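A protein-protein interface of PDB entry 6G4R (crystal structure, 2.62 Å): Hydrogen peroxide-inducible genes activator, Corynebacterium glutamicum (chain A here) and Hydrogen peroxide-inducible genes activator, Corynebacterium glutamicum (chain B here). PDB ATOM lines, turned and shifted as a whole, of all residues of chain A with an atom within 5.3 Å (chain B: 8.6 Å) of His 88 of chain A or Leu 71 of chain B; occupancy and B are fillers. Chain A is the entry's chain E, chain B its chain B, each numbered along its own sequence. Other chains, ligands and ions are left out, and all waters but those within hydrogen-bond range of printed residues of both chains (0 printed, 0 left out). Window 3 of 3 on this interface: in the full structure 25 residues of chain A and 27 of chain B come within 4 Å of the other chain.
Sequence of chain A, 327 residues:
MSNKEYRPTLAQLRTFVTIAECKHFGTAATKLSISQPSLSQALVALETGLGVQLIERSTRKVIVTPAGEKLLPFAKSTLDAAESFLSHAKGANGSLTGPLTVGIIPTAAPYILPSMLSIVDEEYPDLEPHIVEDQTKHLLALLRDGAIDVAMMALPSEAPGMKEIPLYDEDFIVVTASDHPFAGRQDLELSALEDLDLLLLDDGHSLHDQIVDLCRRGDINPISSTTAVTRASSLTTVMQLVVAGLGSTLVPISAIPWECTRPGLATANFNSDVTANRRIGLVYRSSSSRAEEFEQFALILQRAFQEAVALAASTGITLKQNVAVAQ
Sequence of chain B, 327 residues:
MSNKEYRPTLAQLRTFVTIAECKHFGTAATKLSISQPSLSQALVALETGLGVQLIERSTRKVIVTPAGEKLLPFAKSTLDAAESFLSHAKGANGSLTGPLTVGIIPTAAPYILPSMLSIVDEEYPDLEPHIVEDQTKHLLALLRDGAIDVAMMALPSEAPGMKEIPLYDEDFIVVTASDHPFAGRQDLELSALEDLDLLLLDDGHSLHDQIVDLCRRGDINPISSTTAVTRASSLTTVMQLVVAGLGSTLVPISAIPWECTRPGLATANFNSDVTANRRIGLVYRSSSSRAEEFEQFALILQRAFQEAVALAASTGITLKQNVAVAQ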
ATOM      1  N   SER A  84     -20.140   4.516  -8.401  1.00  0.00           N
ATOM      2  CA  SER A  84     -21.202   3.983  -7.557  1.00  0.00           C
ATOM      3  C   SER A  84     -21.354   4.792  -6.279  1.00  0.00           C
ATOM      4  O   SER A  84     -22.457   4.877  -5.732  1.00  0.00           O
ATOM      5  CB  SER A  84     -20.945   2.516  -7.196  1.00  0.00           C
ATOM      6  OG  SER A  84     -19.739   2.375  -6.459  1.00  0.00           O
ATOM      7  N   PHE A  85     -20.260   5.370  -5.781  1.00  0.00           N
ATOM      8  CA  PHE A  85     -20.336   6.220  -4.596  1.00  0.00           C
ATOM      9  C   PHE A  85     -21.076   7.522  -4.890  1.00  0.00           C
ATOM     10  O   PHE A  85     -21.902   7.966  -4.083  1.00  0.00           O
ATOM     11  CB  PHE A  85     -18.928   6.503  -4.063  1.00  0.00           C
ATOM     12  CG  PHE A  85     -18.896   7.479  -2.908  1.00  0.00           C
ATOM     13  CD1 PHE A  85     -19.148   7.051  -1.615  1.00  0.00           C
ATOM     14  CD2 PHE A  85     -18.585   8.817  -3.112  1.00  0.00           C
ATOM     15  CE1 PHE A  85     -19.117   7.941  -0.548  1.00  0.00           C
ATOM     16  CE2 PHE A  85     -18.550   9.713  -2.047  1.00  0.00           C
ATOM     17  CZ  PHE A  85     -18.816   9.272  -0.764  1.00  0.00           C
ATOM     18  N   LEU A  86     -20.796   8.150  -6.038  1.00  0.00           N
ATOM     19  CA  LEU A  86     -21.478   9.391  -6.392  1.00  0.00           C
ATOM     20  C   LEU A  86     -22.958   9.167  -6.682  1.00  0.00           C
ATOM     21  O   LEU A  86     -23.776  10.063  -6.439  1.00  0.00           O
ATOM     22  CB  LEU A  86     -20.794  10.042  -7.595  1.00  0.00           C
ATOM     23  CG  LEU A  86     -21.295  11.422  -8.033  1.00  0.00           C
ATOM     24  CD1 LEU A  86     -21.160  12.433  -6.903  1.00  0.00           C
ATOM     25  CD2 LEU A  86     -20.548  11.898  -9.271  1.00  0.00           C
ATOM     26  N   SER A  87     -23.320   7.992  -7.201  1.00  0.00           N
ATOM     27  CA  SER A  87     -24.723   7.706  -7.482  1.00  0.00           C
ATOM     28  C   SER A  87     -25.541   7.628  -6.199  1.00  0.00           C
ATOM     29  O   SER A  87     -26.648   8.177  -6.125  1.00  0.00           O
ATOM     30  CB  SER A  87     -24.843   6.405  -8.276  1.00  0.00           C
ATOM     31  OG  SER A  87     -24.210   6.520  -9.538  1.00  0.00           O
ATOM     32  N   HIS A  88     -25.015   6.951  -5.177  1.00  0.00           N
ATOM     33  CA  HIS A  88     -25.736   6.833  -3.916  1.00  0.00           C
ATOM     34  C   HIS A  88     -25.682   8.116  -3.100  1.00  0.00           C
ATOM     35  O   HIS A  88     -26.586   8.370  -2.296  1.00  0.00           O
ATOM     36  CB  HIS A  88     -25.181   5.663  -3.102  1.00  0.00           C
ATOM     37  CG  HIS A  88     -25.410   4.328  -3.737  1.00  0.00           C
ATOM     38  ND1 HIS A  88     -24.538   3.779  -4.652  1.00  0.00           N
ATOM     39  CD2 HIS A  88     -26.415   3.433  -3.592  1.00  0.00           C
ATOM     40  CE1 HIS A  88     -24.995   2.603  -5.044  1.00  0.00           C
ATOM     41  NE2 HIS A  88     -26.133   2.368  -4.414  1.00  0.00           N
ATOM     42  N   ALA A  89     -24.641   8.932  -3.282  1.00  0.00           N
ATOM     43  CA  ALA A  89     -24.592  10.214  -2.589  1.00  0.00           C
ATOM     44  C   ALA A  89     -25.663  11.170  -3.095  1.00  0.00           C
ATOM     45  O   ALA A  89     -26.156  12.007  -2.331  1.00  0.00           O
ATOM     46  CB  ALA A  89     -23.208  10.842  -2.739  1.00  0.00           C
ATOM     47  N   LYS A  90     -26.035  11.066  -4.371  1.00  0.00           N
ATOM     48  CA  LYS A  90     -27.078  11.912  -4.948  1.00  0.00           C
ATOM     49  C   LYS A  90     -28.490  11.421  -4.638  1.00  0.00           C
ATOM     50  O   LYS A  90     -29.373  11.464  -5.499  1.00  0.00           O
ATOM     51  CB  LYS A  90     -26.855  12.039  -6.452  1.00  0.00           C
ATOM     52  CG  LYS A  90     -25.557  12.758  -6.794  1.00  0.00           C
ATOM     53  CD  LYS A  90     -25.615  13.446  -8.146  1.00  0.00           C
ATOM     54  CE  LYS A  90     -24.363  14.281  -8.378  1.00  0.00           C
ATOM     55  NZ  LYS A  90     -24.431  15.068  -9.639  1.00  0.00           N
ATOM     56  N   GLY A  91     -28.722  10.942  -3.417  1.00  0.00           N
ATOM     57  CA  GLY A  91     -30.043  10.537  -2.980  1.00  0.00           C
ATOM     58  C   GLY A  91     -30.652   9.327  -3.659  1.00  0.00           C
ATOM     59  O   GLY A  91     -31.815   9.374  -4.073  1.00  0.00           O
ATOM     60  N   ALA A  92     -29.884   8.243  -3.795  1.00  0.00           N
ATOM     61  CA  ALA A  92     -30.409   7.049  -4.451  1.00  0.00           C
ATOM     62  C   ALA A  92     -31.557   6.453  -3.645  1.00  0.00           C
ATOM     63  O   ALA A  92     -32.606   6.103  -4.198  1.00  0.00           O
ATOM     64  CB  ALA A  92     -29.294   6.022  -4.651  1.00  0.00           C
ATOM     65  N   ASN A  93     -31.363   6.324  -2.330  1.00  0.00           N
ATOM     66  CA  ASN A  93     -32.416   5.938  -1.388  1.00  0.00           C
ATOM     67  C   ASN A  93     -32.956   4.537  -1.680  1.00  0.00           C
ATOM     68  O   ASN A  93     -34.162   4.323  -1.818  1.00  0.00           O
ATOM     69  CB  ASN A  93     -33.542   6.976  -1.371  1.00  0.00           C
ATOM     70  CG  ASN A  93     -33.074   8.330  -0.867  1.00  0.00           C
ATOM     71  OD1 ASN A  93     -31.875   8.610  -0.829  1.00  0.00           O
ATOM     72  ND2 ASN A  93     -34.019   9.175  -0.475  1.00  0.00           N
ATOM     73  N   SER A  95     -32.096   1.897  -4.220  1.00  0.00           N
ATOM     74  CA  SER A  95     -32.434   1.414  -5.551  1.00  0.00           C
ATOM     75  C   SER A  95     -31.382   0.428  -6.038  1.00  0.00           C
ATOM     76  O   SER A  95     -30.179   0.691  -5.934  1.00  0.00           O
ATOM     77  CB  SER A  95     -32.550   2.580  -6.535  1.00  0.00           C
ATOM     78  OG  SER A  95     -31.316   3.272  -6.647  1.00  0.00           O
ATOM     79  N   THR A  97     -28.996  -0.647  -8.054  1.00  0.00           N
ATOM     80  CA  THR A  97     -28.080  -0.235  -9.107  1.00  0.00           C
ATOM     81  C   THR A  97     -26.677  -0.714  -8.760  1.00  0.00           C
ATOM     82  O   THR A  97     -26.354  -0.972  -7.598  1.00  0.00           O
ATOM     83  CB  THR A  97     -28.076   1.289  -9.323  1.00  0.00           C
ATOM     84  OG1 THR A  97     -27.747   1.954  -8.098  1.00  0.00           O
ATOM     85  CG2 THR A  97     -29.434   1.771  -9.818  1.00  0.00           C
ATOM     86  N   SER A 289     -25.289  -1.178   5.918  1.00  0.00           N
ATOM     87  CA  SER A 289     -26.248  -0.081   5.911  1.00  0.00           C
ATOM     88  C   SER A 289     -27.187  -0.154   4.716  1.00  0.00           C
ATOM     89  O   SER A 289     -27.916   0.807   4.448  1.00  0.00           O
ATOM     90  CB  SER A 289     -25.516   1.262   5.920  1.00  0.00           C
ATOM     91  OG  SER A 289     -24.598   1.347   4.842  1.00  0.00           O
ATOM     92  N   GLU A 293     -31.986  -1.596   0.632  1.00  0.00           N
ATOM     93  CA  GLU A 293     -31.637  -2.100  -0.690  1.00  0.00           C
ATOM     94  C   GLU A 293     -31.823  -3.610  -0.771  1.00  0.00           C
ATOM     95  O   GLU A 293     -32.221  -4.134  -1.817  1.00  0.00           O
ATOM     96  CB  GLU A 293     -30.199  -1.715  -1.038  1.00  0.00           C
ATOM     97  CG  GLU A 293     -29.755  -2.164  -2.421  1.00  0.00           C
ATOM     98  CD  GLU A 293     -28.329  -1.760  -2.738  1.00  0.00           C
ATOM     99  OE1 GLU A 293     -27.729  -1.010  -1.939  1.00  0.00           O
ATOM    100  OE2 GLU A 293     -27.808  -2.194  -3.787  1.00  0.00           O
ATOM    101  N   LEU B  13     -11.922  10.476   0.177  1.00  0.00           N
ATOM    102  CA  LEU B  13     -12.561   9.245   0.631  1.00  0.00           C
ATOM    103  C   LEU B  13     -11.735   8.566   1.715  1.00  0.00           C
ATOM    104  O   LEU B  13     -12.288   8.058   2.697  1.00  0.00           O
ATOM    105  CB  LEU B  13     -12.778   8.302  -0.552  1.00  0.00           C
ATOM    106  CG  LEU B  13     -13.704   8.808  -1.660  1.00  0.00           C
ATOM    107  CD1 LEU B  13     -13.748   7.825  -2.819  1.00  0.00           C
ATOM    108  CD2 LEU B  13     -15.101   9.060  -1.113  1.00  0.00           C
ATOM    109  N   PHE B  16     -12.532  10.338   4.916  1.00  0.00           N
ATOM    110  CA  PHE B  16     -13.871  10.090   5.445  1.00  0.00           C
ATOM    111  C   PHE B  16     -13.982   8.702   6.063  1.00  0.00           C
ATOM    112  O   PHE B  16     -14.651   8.525   7.088  1.00  0.00           O
ATOM    113  CB  PHE B  16     -14.910  10.274   4.338  1.00  0.00           C
ATOM    114  CG  PHE B  16     -16.277   9.769   4.699  1.00  0.00           C
ATOM    115  CD1 PHE B  16     -16.849   8.720   3.997  1.00  0.00           C
ATOM    116  CD2 PHE B  16     -16.990  10.336   5.742  1.00  0.00           C
ATOM    117  CE1 PHE B  16     -18.107   8.251   4.324  1.00  0.00           C
ATOM    118  CE2 PHE B  16     -18.249   9.870   6.075  1.00  0.00           C
ATOM    119  CZ  PHE B  16     -18.808   8.827   5.365  1.00  0.00           C
ATOM    120  N   VAL B  17     -13.338   7.703   5.455  1.00  0.00           N
ATOM    121  CA  VAL B  17     -13.405   6.348   5.994  1.00  0.00           C
ATOM    122  C   VAL B  17     -12.663   6.256   7.322  1.00  0.00           C
ATOM    123  O   VAL B  17     -13.154   5.649   8.282  1.00  0.00           O
ATOM    124  CB  VAL B  17     -12.856   5.341   4.968  1.00  0.00           C
ATOM    125  CG1 VAL B  17     -12.782   3.950   5.577  1.00  0.00           C
ATOM    126  CG2 VAL B  17     -13.723   5.331   3.720  1.00  0.00           C
ATOM    127  N   ALA B  20     -14.625   7.819  10.248  1.00  0.00           N
ATOM    128  CA  ALA B  20     -15.789   7.055  10.685  1.00  0.00           C
ATOM    129  C   ALA B  20     -15.401   5.847  11.529  1.00  0.00           C
ATOM    130  O   ALA B  20     -16.178   5.425  12.394  1.00  0.00           O
ATOM    131  CB  ALA B  20     -16.606   6.609   9.474  1.00  0.00           C
ATOM    132  N   LEU B  46     -15.121  17.381   0.894  1.00  0.00           N
ATOM    133  CA  LEU B  46     -16.008  16.296   0.489  1.00  0.00           C
ATOM    134  C   LEU B  46     -17.455  16.605   0.850  1.00  0.00           C
ATOM    135  O   LEU B  46     -18.370  16.323   0.066  1.00  0.00           O
ATOM    136  CB  LEU B  46     -15.558  14.984   1.135  1.00  0.00           C
ATOM    137  CG  LEU B  46     -16.354  13.731   0.769  1.00  0.00           C
ATOM    138  CD1 LEU B  46     -16.231  13.432  -0.716  1.00  0.00           C
ATOM    139  CD2 LEU B  46     -15.888  12.544   1.596  1.00  0.00           C
ATOM    140  N   LEU B  50     -20.374  17.409  -2.147  1.00  0.00           N
ATOM    141  CA  LEU B  50     -21.580  16.598  -2.233  1.00  0.00           C
ATOM    142  C   LEU B  50     -22.813  17.295  -1.676  1.00  0.00           C
ATOM    143  O   LEU B  50     -23.933  16.887  -2.001  1.00  0.00           O
ATOM    144  CB  LEU B  50     -21.381  15.270  -1.492  1.00  0.00           C
ATOM    145  CG  LEU B  50     -20.201  14.406  -1.940  1.00  0.00           C
ATOM    146  CD1 LEU B  50     -20.063  13.184  -1.044  1.00  0.00           C
ATOM    147  CD2 LEU B  50     -20.360  13.993  -3.394  1.00  0.00           C
ATOM    148  N   VAL B  52     -23.858  17.432   1.543  1.00  0.00           N
ATOM    149  CA  VAL B  52     -24.497  16.625   2.574  1.00  0.00           C
ATOM    150  C   VAL B  52     -23.593  16.579   3.797  1.00  0.00           C
ATOM    151  O   VAL B  52     -22.364  16.615   3.688  1.00  0.00           O
ATOM    152  CB  VAL B  52     -24.810  15.193   2.083  1.00  0.00           C
ATOM    153  CG1 VAL B  52     -26.043  15.185   1.192  1.00  0.00           C
ATOM    154  CG2 VAL B  52     -23.611  14.609   1.353  1.00  0.00           C
ATOM    155  N   GLN B  53     -24.216  16.501   4.971  1.00  0.00           N
ATOM    156  CA  GLN B  53     -23.487  16.410   6.232  1.00  0.00           C
ATOM    157  C   GLN B  53     -23.107  14.955   6.475  1.00  0.00           C
ATOM    158  O   GLN B  53     -23.976  14.113   6.721  1.00  0.00           O
ATOM    159  CB  GLN B  53     -24.334  16.960   7.377  1.00  0.00           C
ATOM    160  CG  GLN B  53     -23.705  16.825   8.758  1.00  0.00           C
ATOM    161  CD  GLN B  53     -22.640  17.871   9.031  1.00  0.00           C
ATOM    162  OE1 GLN B  53     -22.261  18.639   8.147  1.00  0.00           O
ATOM    163  NE2 GLN B  53     -22.153  17.907  10.266  1.00  0.00           N
ATOM    164  N   LEU B  54     -21.810  14.656   6.405  1.00  0.00           N
ATOM    165  CA  LEU B  54     -21.336  13.287   6.574  1.00  0.00           C
ATOM    166  C   LEU B  54     -20.962  12.957   8.012  1.00  0.00           C
ATOM    167  O   LEU B  54     -21.148  11.814   8.444  1.00  0.00           O
ATOM    168  CB  LEU B  54     -20.128  13.031   5.671  1.00  0.00           C
ATOM    169  CG  LEU B  54     -20.411  12.847   4.180  1.00  0.00           C
ATOM    170  CD1 LEU B  54     -19.120  12.590   3.418  1.00  0.00           C
ATOM    171  CD2 LEU B  54     -21.406  11.720   3.955  1.00  0.00           C
ATOM    172  N   VAL B  64     -21.097   9.333  12.976  1.00  0.00           N
ATOM    173  CA  VAL B  64     -21.395   9.359  11.550  1.00  0.00           C
ATOM    174  C   VAL B  64     -22.878   9.651  11.364  1.00  0.00           C
ATOM    175  O   VAL B  64     -23.729   9.052  12.031  1.00  0.00           O
ATOM    176  CB  VAL B  64     -21.000   8.031  10.886  1.00  0.00           C
ATOM    177  CG1 VAL B  64     -21.102   8.143   9.373  1.00  0.00           C
ATOM    178  CG2 VAL B  64     -19.596   7.628  11.305  1.00  0.00           C
ATOM    179  N   THR B  65     -23.188  10.578  10.462  1.00  0.00           N
ATOM    180  CA  THR B  65     -24.566  10.971  10.234  1.00  0.00           C
ATOM    181  C   THR B  65     -25.331   9.841   9.549  1.00  0.00           C
ATOM    182  O   THR B  65     -24.728   8.925   8.986  1.00  0.00           O
ATOM    183  CB  THR B  65     -24.620  12.239   9.384  1.00  0.00           C
ATOM    184  OG1 THR B  65     -24.004  11.990   8.115  1.00  0.00           O
ATOM    185  CG2 THR B  65     -23.892  13.377  10.083  1.00  0.00           C
ATOM    186  N   PRO B  66     -26.669   9.870   9.608  1.00  0.00           N
ATOM    187  CA  PRO B  66     -27.452   8.867   8.862  1.00  0.00           C
ATOM    188  C   PRO B  66     -27.067   8.766   7.393  1.00  0.00           C
ATOM    189  O   PRO B  66     -26.927   7.655   6.867  1.00  0.00           O
ATOM    190  CB  PRO B  66     -28.894   9.352   9.049  1.00  0.00           C
ATOM    191  CG  PRO B  66     -28.881  10.076  10.348  1.00  0.00           C
ATOM    192  CD  PRO B  66     -27.514  10.683  10.503  1.00  0.00           C
ATOM    193  N   ALA B  67     -26.895   9.903   6.713  1.00  0.00           N
ATOM    194  CA  ALA B  67     -26.456   9.869   5.322  1.00  0.00           C
ATOM    195  C   ALA B  67     -25.038   9.324   5.196  1.00  0.00           C
ATOM    196  O   ALA B  67     -24.712   8.680   4.192  1.00  0.00           O
ATOM    197  CB  ALA B  67     -26.547  11.265   4.705  1.00  0.00           C
ATOM    198  N   GLY B  68     -24.189   9.570   6.196  1.00  0.00           N
ATOM    199  CA  GLY B  68     -22.836   9.044   6.155  1.00  0.00           C
ATOM    200  C   GLY B  68     -22.779   7.535   6.278  1.00  0.00           C
ATOM    201  O   GLY B  68     -21.910   6.893   5.678  1.00  0.00           O
ATOM    202  N   GLU B  69     -23.689   6.950   7.061  1.00  0.00           N
ATOM    203  CA  GLU B  69     -23.700   5.500   7.233  1.00  0.00           C
ATOM    204  C   GLU B  69     -24.008   4.786   5.923  1.00  0.00           C
ATOM    205  O   GLU B  69     -23.438   3.726   5.636  1.00  0.00           O
ATOM    206  CB  GLU B  69     -24.717   5.110   8.306  1.00  0.00           C
ATOM    207  CG  GLU B  69     -24.337   5.543   9.712  1.00  0.00           C
ATOM    208  CD  GLU B  69     -25.503   5.465  10.680  1.00  0.00           C
ATOM    209  OE1 GLU B  69     -26.619   5.879  10.301  1.00  0.00           O
ATOM    210  OE2 GLU B  69     -25.304   4.988  11.817  1.00  0.00           O
ATOM    211  N   LYS B  70     -24.905   5.352   5.111  1.00  0.00           N
ATOM    212  CA  LYS B  70     -25.255   4.717   3.844  1.00  0.00           C
ATOM    213  C   LYS B  70     -24.115   4.796   2.836  1.00  0.00           C
ATOM    214  O   LYS B  70     -23.976   3.907   1.989  1.00  0.00           O
ATOM    215  CB  LYS B  70     -26.519   5.354   3.264  1.00  0.00           C
ATOM    216  CG  LYS B  70     -27.705   5.360   4.215  1.00  0.00           C
ATOM    217  CD  LYS B  70     -29.023   5.426   3.455  1.00  0.00           C
ATOM    218  CE  LYS B  70     -29.066   6.621   2.514  1.00  0.00           C
ATOM    219  NZ  LYS B  70     -28.909   7.914   3.236  1.00  0.00           N
ATOM    220  N   LEU B  71     -23.296   5.845   2.906  1.00  0.00           N
ATOM    221  CA  LEU B  71     -22.218   6.042   1.946  1.00  0.00           C
ATOM    222  C   LEU B  71     -20.923   5.347   2.335  1.00  0.00           C
ATOM    223  O   LEU B  71     -20.101   5.069   1.455  1.00  0.00           O
ATOM    224  CB  LEU B  71     -21.945   7.537   1.758  1.00  0.00           C
ATOM    225  CG  LEU B  71     -23.041   8.314   1.032  1.00  0.00           C
ATOM    226  CD1 LEU B  71     -22.733   9.802   1.022  1.00  0.00           C
ATOM    227  CD2 LEU B  71     -23.196   7.779  -0.379  1.00  0.00           C
ATOM    228  N   LEU B  72     -20.720   5.073   3.624  1.00  0.00           N
ATOM    229  CA  LEU B  72     -19.464   4.489   4.097  1.00  0.00           C
ATOM    230  C   LEU B  72     -19.077   3.192   3.392  1.00  0.00           C
ATOM    231  O   LEU B  72     -17.903   3.059   3.010  1.00  0.00           O
ATOM    232  CB  LEU B  72     -19.545   4.291   5.617  1.00  0.00           C
ATOM    233  CG  LEU B  72     -18.279   3.773   6.301  1.00  0.00           C
ATOM    234  CD1 LEU B  72     -17.127   4.745   6.103  1.00  0.00           C
ATOM    235  CD2 LEU B  72     -18.531   3.533   7.781  1.00  0.00           C
ATOM    236  N   PRO B  73     -19.968   2.208   3.196  1.00  0.00           N
ATOM    237  CA  PRO B  73     -19.535   0.993   2.481  1.00  0.00           C
ATOM    238  C   PRO B  73     -19.086   1.258   1.055  1.00  0.00           C
ATOM    239  O   PRO B  73     -18.144   0.613   0.576  1.00  0.00           O
ATOM    240  CB  PRO B  73     -20.782   0.098   2.528  1.00  0.00           C
ATOM    241  CG  PRO B  73     -21.565   0.591   3.687  1.00  0.00           C
ATOM    242  CD  PRO B  73     -21.344   2.070   3.706  1.00  0.00           C
ATOM    243  N   PHE B  74     -19.735   2.193   0.358  1.00  0.00           N
ATOM    244  CA  PHE B  74     -19.336   2.498  -1.012  1.00  0.00           C
ATOM    245  C   PHE B  74     -17.975   3.181  -1.065  1.00  0.00           C
ATOM    246  O   PHE B  74     -17.230   2.999  -2.036  1.00  0.00           O
ATOM    247  CB  PHE B  74     -20.400   3.360  -1.690  1.00  0.00           C
ATOM    248  CG  PHE B  74     -21.758   2.721  -1.719  1.00  0.00           C
ATOM    249  CD1 PHE B  74     -22.039   1.702  -2.615  1.00  0.00           C
ATOM    250  CD2 PHE B  74     -22.753   3.136  -0.850  1.00  0.00           C
ATOM    251  CE1 PHE B  74     -23.286   1.108  -2.642  1.00  0.00           C
ATOM    252  CE2 PHE B  74     -24.003   2.547  -0.874  1.00  0.00           C
ATOM    253  CZ  PHE B  74     -24.269   1.532  -1.772  1.00  0.00           C
ATOM    254  N   ALA B  75     -17.634   3.968  -0.043  1.00  0.00           N
ATOM    255  CA  ALA B  75     -16.319   4.596  -0.012  1.00  0.00           C
ATOM    256  C   ALA B  75     -15.221   3.584   0.286  1.00  0.00           C
ATOM    257  O   ALA B  75     -14.109   3.704  -0.243  1.00  0.00           O
ATOM    258  CB  ALA B  75     -16.298   5.723   1.021  1.00  0.00           C
ATOM    259  N   LYS B  76     -15.510   2.581   1.119  1.00  0.00           N
ATOM    260  CA  LYS B  76     -14.500   1.578   1.443  1.00  0.00           C
ATOM    261  C   LYS B  76     -14.236   0.654   0.261  1.00  0.00           C
ATOM    262  O   LYS B  76     -13.090   0.259   0.019  1.00  0.00           O
ATOM    263  CB  LYS B  76     -14.929   0.776   2.672  1.00  0.00           C
ATOM    264  CG  LYS B  76     -14.968   1.593   3.953  1.00  0.00           C
ATOM    265  CD  LYS B  76     -15.181   0.717   5.179  1.00  0.00           C
ATOM    266  CE  LYS B  76     -16.560   0.081   5.176  1.00  0.00           C
ATOM    267  NZ  LYS B  76     -16.793  -0.732   6.403  1.00  0.00           N
ATOM    268  N   SER B  77     -15.284   0.294  -0.487  1.00  0.00           N
ATOM    269  CA  SER B  77     -15.084  -0.524  -1.679  1.00  0.00           C
ATOM    270  C   SER B  77     -14.325   0.237  -2.758  1.00  0.00           C
ATOM    271  O   SER B  77     -13.606  -0.376  -3.556  1.00  0.00           O
ATOM    272  CB  SER B  77     -16.430  -1.013  -2.214  1.00  0.00           C
ATOM    273  OG  SER B  77     -17.322   0.068  -2.414  1.00  0.00           O
ATOM    274  N   THR B  78     -14.475   1.563  -2.803  1.00  0.00           N
ATOM    275  CA  THR B  78     -13.688   2.364  -3.735  1.00  0.00           C
ATOM    276  C   THR B  78     -12.209   2.338  -3.371  1.00  0.00           C
ATOM    277  O   THR B  78     -11.348   2.231  -4.253  1.00  0.00           O
ATOM    278  CB  THR B  78     -14.208   3.803  -3.764  1.00  0.00           C
ATOM    279  OG1 THR B  78     -15.606   3.802  -4.077  1.00  0.00           O
ATOM    280  CG2 THR B  78     -13.464   4.618  -4.811  1.00  0.00           C
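The backbone carbonyl oxygen (O) of Glu 69 of chain B lies within hydrogen-bond range of the side-chain hydroxyl (OG) of Ser 289 of chain A (2.8 Å).
O of Pro 73 of chain B lies within hydrogen-bond range of OG of Ser 77 of chain B (3.1 Å). The backbone carbonyl oxygen (O) of Phe 74 of chain B sits at hydrogen-bond distance from the side-chain hydroxyl (OG) of Ser 77 of chain B (3.0 Å). The backbone carbonyl oxygen (O) of Phe 74 of chain B lies within hydrogen-bond range of the side-chain hydroxyl (OG1) of Thr 78 of chain B, 2.7 Å away. A ring nitrogen (ND1) of His 88 of chain A sits at hydrogen-bond distance from the backbone carbonyl oxygen (O) of Ser 84 of chain A, at 2.6 Å.
Phe 85 of chain A touches Leu 13 of chain B (CE2 to CD2, 3.6 Å). Phe 85 of chain A touches Leu 50 of chain B. Leu 71 of chain B touches Phe 85 of chain A. Phe 85 of chain A touches Phe 74 of chain B. CD1 of Phe 85 of chain A touches N of Ala 75 of chain B (3.8 Å). Leu 50 of chain B touches Leu 86 of chain A. CD2 of Leu 71 of chain B touches C of His 88 of chain A (3.7 Å). CD2 of Leu 71 of chain B touches N of Ala 89 of chain A (3.4 Å). Ser 289 of chain A touches Lys 70 of chain B. Ser 289 of chain A touches Pro 73 of chain B (OG to CG, 3.3 Å).
Printed residues of chain B within 4 Å of Phe 85 of chain A: Leu 13 (3.6 Å), Leu 50 (3.9 Å), Leu 71 (3.6 Å), Phe 74 (3.9 Å) and Ala 75 (3.8 Å). His 88 of chain A touches just these residues of chain B: Leu 71 and Phe 74. Of chain B, only Leu 71 (3.4 Å) comes within 4 Å of Ala 89 of chain A. Gly 91 of chain A touches none of the printed residues of chain B. Leu 71 of chain B touches just these residues of chain A: Phe 85, His 88 and Ala 89. Printed residues of chain A within 4 Å of Ala 75 of chain B: Phe 85. The nearest residue of chain B that does not touch His 88 of chain A is Lys 70 of chain B (5.5 Å). The nearest residue of chain A that does not touch Leu 71 of chain B is Ser 289 of chain A (5.1 Å).
Of the 24 printed residues of chain B, 8 touch a printed residue of chain A. Printed residues of chain B that touch a printed residue of chain A: Leu 13, Leu 50, Glu 69, Lys 70, Leu 71, Pro 73, Phe 74 and Ala 75. Hydrophobic or aromatic side chains of chain B that line the printed part of chain A: Leu 13, Leu 50, Leu 71, Pro 73, Phe 74 and Ala 75. Hydrophobic or aromatic side chains of chain A within 4 Å of the printed part of chain B: Phe 85, Leu 86, His 88 and Ala 89.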
